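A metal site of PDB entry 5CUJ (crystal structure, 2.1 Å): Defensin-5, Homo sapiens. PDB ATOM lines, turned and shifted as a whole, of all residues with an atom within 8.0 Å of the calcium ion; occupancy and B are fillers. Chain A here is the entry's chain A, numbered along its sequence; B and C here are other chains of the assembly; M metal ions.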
ATOM      1  N   CYS A  20     -16.151  27.771  -5.378  1.00  0.00           N
ATOM      2  CA  CYS A  20     -17.312  26.932  -5.688  1.00  0.00           C
ATOM      3  C   CYS A  20     -17.032  25.531  -5.122  1.00  0.00           C
ATOM      4  O   CYS A  20     -16.054  25.344  -4.392  1.00  0.00           O
ATOM      5  CB  CYS A  20     -17.565  26.897  -7.197  1.00  0.00           C
ATOM      6  SG  CYS A  20     -16.131  26.388  -8.172  1.00  0.00           S
ATOM      7  N   GLU A  21     -17.879  24.556  -5.452  1.00  0.00           N
ATOM      8  CA  GLU A  21     -17.681  23.191  -4.946  1.00  0.00           C
ATOM      9  C   GLU A  21     -17.873  22.112  -6.000  1.00  0.00           C
ATOM     10  O   GLU A  21     -18.831  22.146  -6.772  1.00  0.00           O
ATOM     11  CB  GLU A  21     -18.606  22.931  -3.763  1.00  0.00           C
ATOM     12  CG  GLU A  21     -18.017  23.348  -2.424  1.00  0.00           C
ATOM     13  CD  GLU A  21     -18.879  22.906  -1.257  1.00  0.00           C
ATOM     14  OE1 GLU A  21     -20.118  22.889  -1.393  1.00  0.00           O
ATOM     15  OE2 GLU A  21     -18.312  22.587  -0.188  1.00  0.00           O
ATOM     16  N   ILE A  22     -16.949  21.146  -5.995  1.00  0.00           N
ATOM     17  CA  ILE A  22     -17.054  19.933  -6.801  1.00  0.00           C
ATOM     18  C   ILE A  22     -17.157  18.749  -5.848  1.00  0.00           C
ATOM     19  O   ILE A  22     -16.172  18.377  -5.196  1.00  0.00           O
ATOM     20  CB  ILE A  22     -15.838  19.785  -7.742  1.00  0.00           C
ATOM     21  CG1 ILE A  22     -15.817  20.945  -8.747  1.00  0.00           C
ATOM     22  CG2 ILE A  22     -15.867  18.440  -8.454  1.00  0.00           C
ATOM     23  CD1 ILE A  22     -14.552  21.058  -9.547  1.00  0.00           C
ATOM     24  N   SER A  23     -18.354  18.182  -5.750  1.00  0.00           N
ATOM     25  CA  SER A  23     -18.650  17.060  -4.849  1.00  0.00           C
ATOM     26  C   SER A  23     -18.249  17.350  -3.404  1.00  0.00           C
ATOM     27  O   SER A  23     -17.514  16.581  -2.782  1.00  0.00           O
ATOM     28  CB  SER A  23     -18.001  15.762  -5.351  1.00  0.00           C
ATOM     29  OG  SER A  23     -18.680  15.317  -6.499  1.00  0.00           O
ATOM     30  N   GLY A  24     -18.713  18.489  -2.898  1.00  0.00           N
ATOM     31  CA  GLY A  24     -18.462  18.885  -1.527  1.00  0.00           C
ATOM     32  C   GLY A  24     -17.030  19.270  -1.194  1.00  0.00           C
ATOM     33  O   GLY A  24     -16.686  19.373  -0.011  1.00  0.00           O
ATOM     34  N   ARG A  25     -16.188  19.487  -2.206  1.00  0.00           N
ATOM     35  CA  ARG A  25     -14.813  19.924  -2.008  1.00  0.00           C
ATOM     36  C   ARG A  25     -14.632  21.289  -2.654  1.00  0.00           C
ATOM     37  O   ARG A  25     -15.184  21.537  -3.728  1.00  0.00           O
ATOM     38  CB  ARG A  25     -13.834  18.903  -2.593  1.00  0.00           C
ATOM     39  CG  ARG A  25     -13.944  17.524  -1.964  1.00  0.00           C
ATOM     40  CD  ARG A  25     -12.725  16.644  -2.247  1.00  0.00           C
ATOM     41  NE  ARG A  25     -11.808  16.579  -1.111  1.00  0.00           N
ATOM     42  CZ  ARG A  25     -12.014  15.879   0.010  1.00  0.00           C
ATOM     43  NH1 ARG A  25     -13.127  15.170   0.197  1.00  0.00           N
ATOM     44  NH2 ARG A  25     -11.084  15.900   0.976  1.00  0.00           N
ATOM     45  N   LEU A  26     -13.865  22.156  -1.996  1.00  0.00           N
ATOM     46  CA  LEU A  26     -13.665  23.525  -2.469  1.00  0.00           C
ATOM     47  C   LEU A  26     -12.871  23.508  -3.768  1.00  0.00           C
ATOM     48  O   LEU A  26     -11.823  22.860  -3.856  1.00  0.00           O
ATOM     49  CB  LEU A  26     -12.928  24.386  -1.441  1.00  0.00           C
ATOM     50  CG  LEU A  26     -13.587  24.595  -0.078  1.00  0.00           C
ATOM     51  CD1 LEU A  26     -12.710  25.505   0.772  1.00  0.00           C
ATOM     52  CD2 LEU A  26     -14.992  25.150  -0.201  1.00  0.00           C
ATOM     53  N   CYS B  20     -22.388  28.395   6.038  1.00  0.00           N
ATOM     54  CA  CYS B  20     -22.362  27.182   6.840  1.00  0.00           C
ATOM     55  C   CYS B  20     -22.338  26.001   5.876  1.00  0.00           C
ATOM     56  O   CYS B  20     -22.198  26.199   4.656  1.00  0.00           O
ATOM     57  CB  CYS B  20     -23.586  27.149   7.770  1.00  0.00           C
ATOM     58  SG  CYS B  20     -25.157  27.371   6.904  1.00  0.00           S
ATOM     59  N   GLU B  21     -22.465  24.778   6.393  1.00  0.00           N
ATOM     60  CA  GLU B  21     -22.467  23.572   5.555  1.00  0.00           C
ATOM     61  C   GLU B  21     -23.590  22.605   5.883  1.00  0.00           C
ATOM     62  O   GLU B  21     -23.954  22.435   7.056  1.00  0.00           O
ATOM     63  CB  GLU B  21     -21.121  22.852   5.674  1.00  0.00           C
ATOM     64  CG  GLU B  21     -20.098  23.265   4.634  1.00  0.00           C
ATOM     65  CD  GLU B  21     -18.873  22.379   4.659  1.00  0.00           C
ATOM     66  OE1 GLU B  21     -18.480  21.926   5.755  1.00  0.00           O
ATOM     67  OE2 GLU B  21     -18.292  22.134   3.576  1.00  0.00           O
ATOM     68  N   ILE B  22     -24.126  21.957   4.841  1.00  0.00           N
ATOM     69  CA  ILE B  22     -25.133  20.907   4.976  1.00  0.00           C
ATOM     70  C   ILE B  22     -24.595  19.674   4.254  1.00  0.00           C
ATOM     71  O   ILE B  22     -24.599  19.619   3.023  1.00  0.00           O
ATOM     72  CB  ILE B  22     -26.491  21.355   4.393  1.00  0.00           C
ATOM     73  CG1 ILE B  22     -27.053  22.504   5.249  1.00  0.00           C
ATOM     74  CG2 ILE B  22     -27.477  20.201   4.348  1.00  0.00           C
ATOM     75  CD1 ILE B  22     -28.303  23.151   4.693  1.00  0.00           C
ATOM     76  N   SER B  23     -24.146  18.683   5.031  1.00  0.00           N
ATOM     77  CA  SER B  23     -23.489  17.475   4.512  1.00  0.00           C
ATOM     78  C   SER B  23     -22.331  17.807   3.569  1.00  0.00           C
ATOM     79  O   SER B  23     -22.305  17.390   2.408  1.00  0.00           O
ATOM     80  CB  SER B  23     -24.491  16.531   3.850  1.00  0.00           C
ATOM     81  OG  SER B  23     -25.254  15.872   4.838  1.00  0.00           O
ATOM     82  N   GLY B  24     -21.398  18.592   4.088  1.00  0.00           N
ATOM     83  CA  GLY B  24     -20.202  18.978   3.340  1.00  0.00           C
ATOM     84  C   GLY B  24     -20.440  19.800   2.092  1.00  0.00           C
ATOM     85  O   GLY B  24     -19.544  19.903   1.259  1.00  0.00           O
ATOM     86  N   ARG B  25     -21.623  20.408   1.966  1.00  0.00           N
ATOM     87  CA  ARG B  25     -21.933  21.293   0.847  1.00  0.00           C
ATOM     88  C   ARG B  25     -22.228  22.676   1.400  1.00  0.00           C
ATOM     89  O   ARG B  25     -22.824  22.801   2.472  1.00  0.00           O
ATOM     90  CB  ARG B  25     -23.127  20.756   0.051  1.00  0.00           C
ATOM     91  CG  ARG B  25     -22.826  19.455  -0.678  1.00  0.00           C
ATOM     92  CD  ARG B  25     -23.960  19.022  -1.593  1.00  0.00           C
ATOM     93  NE  ARG B  25     -23.522  17.988  -2.542  1.00  0.00           N
ATOM     94  CZ  ARG B  25     -23.123  18.192  -3.807  1.00  0.00           C
ATOM     95  NH1 ARG B  25     -23.071  19.406  -4.359  1.00  0.00           N
ATOM     96  NH2 ARG B  25     -22.758  17.139  -4.539  1.00  0.00           N
ATOM     97  N   LEU B  26     -21.802  23.727   0.683  1.00  0.00           N
ATOM     98  CA  LEU B  26     -21.967  25.091   1.164  1.00  0.00           C
ATOM     99  C   LEU B  26     -23.425  25.480   1.162  1.00  0.00           C
ATOM    100  O   LEU B  26     -24.151  25.190   0.205  1.00  0.00           O
ATOM    101  CB  LEU B  26     -21.179  26.098   0.312  1.00  0.00           C
ATOM    102  CG  LEU B  26     -19.662  26.006   0.262  1.00  0.00           C
ATOM    103  CD1 LEU B  26     -19.084  27.290  -0.316  1.00  0.00           C
ATOM    104  CD2 LEU B  26     -19.043  25.704   1.623  1.00  0.00           C
ATOM    105  N   CYS C  20      -9.527  25.320   5.474  1.00  0.00           N
ATOM    106  CA  CYS C  20      -9.168  24.138   4.688  1.00  0.00           C
ATOM    107  C   CYS C  20     -10.337  23.161   4.795  1.00  0.00           C
ATOM    108  O   CYS C  20     -11.435  23.559   5.200  1.00  0.00           O
ATOM    109  CB  CYS C  20      -7.857  23.543   5.210  1.00  0.00           C
ATOM    110  SG  CYS C  20      -7.833  23.290   6.996  1.00  0.00           S
ATOM    111  N   GLU C  21     -10.141  21.905   4.393  1.00  0.00           N
ATOM    112  CA  GLU C  21     -11.200  20.900   4.491  1.00  0.00           C
ATOM    113  C   GLU C  21     -10.673  19.553   4.957  1.00  0.00           C
ATOM    114  O   GLU C  21      -9.543  19.165   4.657  1.00  0.00           O
ATOM    115  CB  GLU C  21     -11.920  20.746   3.154  1.00  0.00           C
ATOM    116  CG  GLU C  21     -13.128  21.654   2.997  1.00  0.00           C
ATOM    117  CD  GLU C  21     -13.876  21.412   1.699  1.00  0.00           C
ATOM    118  OE1 GLU C  21     -13.219  21.120   0.673  1.00  0.00           O
ATOM    119  OE2 GLU C  21     -15.118  21.540   1.688  1.00  0.00           O
ATOM    120  N   ILE C  22     -11.522  18.844   5.709  1.00  0.00           N
ATOM    121  CA  ILE C  22     -11.239  17.487   6.154  1.00  0.00           C
ATOM    122  C   ILE C  22     -12.431  16.628   5.741  1.00  0.00           C
ATOM    123  O   ILE C  22     -13.514  16.756   6.310  1.00  0.00           O
ATOM    124  CB  ILE C  22     -11.030  17.415   7.679  1.00  0.00           C
ATOM    125  CG1 ILE C  22      -9.827  18.282   8.074  1.00  0.00           C
ATOM    126  CG2 ILE C  22     -10.828  15.978   8.144  1.00  0.00           C
ATOM    127  CD1 ILE C  22      -9.676  18.495   9.567  1.00  0.00           C
ATOM    128  N   SER C  23     -12.217  15.761   4.754  1.00  0.00           N
ATOM    129  CA  SER C  23     -13.273  14.920   4.164  1.00  0.00           C
ATOM    130  C   SER C  23     -14.458  15.764   3.692  1.00  0.00           C
ATOM    131  O   SER C  23     -15.613  15.477   4.015  1.00  0.00           O
ATOM    132  CB  SER C  23     -13.721  13.827   5.143  1.00  0.00           C
ATOM    133  OG  SER C  23     -12.673  12.910   5.404  1.00  0.00           O
ATOM    134  N   GLY C  24     -14.153  16.833   2.951  1.00  0.00           N
ATOM    135  CA  GLY C  24     -15.174  17.707   2.376  1.00  0.00           C
ATOM    136  C   GLY C  24     -15.916  18.608   3.347  1.00  0.00           C
ATOM    137  O   GLY C  24     -16.931  19.198   2.970  1.00  0.00           O
ATOM    138  N   ARG C  25     -15.419  18.734   4.578  1.00  0.00           N
ATOM    139  CA  ARG C  25     -16.054  19.558   5.597  1.00  0.00           C
ATOM    140  C   ARG C  25     -15.082  20.639   6.072  1.00  0.00           C
ATOM    141  O   ARG C  25     -13.900  20.353   6.276  1.00  0.00           O
ATOM    142  CB  ARG C  25     -16.530  18.694   6.761  1.00  0.00           C
ATOM    143  CG  ARG C  25     -17.651  17.733   6.354  1.00  0.00           C
ATOM    144  CD  ARG C  25     -17.945  16.680   7.405  1.00  0.00           C
ATOM    145  NE  ARG C  25     -18.917  15.696   6.904  1.00  0.00           N
ATOM    146  CZ  ARG C  25     -20.233  15.886   6.810  1.00  0.00           C
ATOM    147  NH1 ARG C  25     -20.812  17.030   7.192  1.00  0.00           N
ATOM    148  NH2 ARG C  25     -21.002  14.908   6.335  1.00  0.00           N
ATOM    149  N   LEU C  26     -15.593  21.858   6.253  1.00  0.00           N
ATOM    150  CA  LEU C  26     -14.744  23.022   6.549  1.00  0.00           C
ATOM    151  C   LEU C  26     -14.029  22.839   7.871  1.00  0.00           C
ATOM    152  O   LEU C  26     -14.646  22.478   8.880  1.00  0.00           O
ATOM    153  CB  LEU C  26     -15.556  24.313   6.612  1.00  0.00           C
ATOM    154  CG  LEU C  26     -16.291  24.767   5.346  1.00  0.00           C
ATOM    155  CD1 LEU C  26     -16.899  26.141   5.583  1.00  0.00           C
ATOM    156  CD2 LEU C  26     -15.377  24.788   4.130  1.00  0.00           C
HETATM  157 CA    CA M   1     -17.463  21.198   1.566  1.00  0.00          CA
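The backbone NH (N) of Leu 26 of chain A sits at hydrogen-bond distance from the side-chain carboxylate (OE1) of Glu 21 of chain C (2.9 Å). The backbone NH (N) of Leu 26 of chain B sits at hydrogen-bond distance from the side-chain carboxylate (OE1) of Glu 21 of chain A (2.8 Å). The side-chain carboxylate (OE1) of Glu 21 of chain B is in hydrogen-bond range of the backbone NH (N) of Leu 26 of chain C, 2.9 Å away.
Six residues have an atom within 4 Å of the calcium ion: Glu 21 of chain A, Gly 24 of chain A, Glu 21 of chain B, Gly 24 of chain B, Glu 21 of chain C and Gly 24 of chain C. Along chain A the residues within 4 Å of the calcium ion span positions 21 to 24. The nearest printed residue that does not touch the calcium ion is Arg 25 of chain B (4.3 Å).
OE2 of Glu 21 of chain B is bound to the calcium ion (2.4 Å). OE2 of Glu 21 of chain C is bound to the calcium ion. OE2 of Glu 21 of chain A binds the calcium ion, 2.4 Å away. O of Gly 24 of chain B is bound to the calcium ion (2.5 Å). The backbone carbonyl oxygen (O) of Gly 24 of chain C binds the calcium ion, 2.5 Å away. O of Gly 24 of chain A is bound to the calcium ion, 2.5 Å away.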
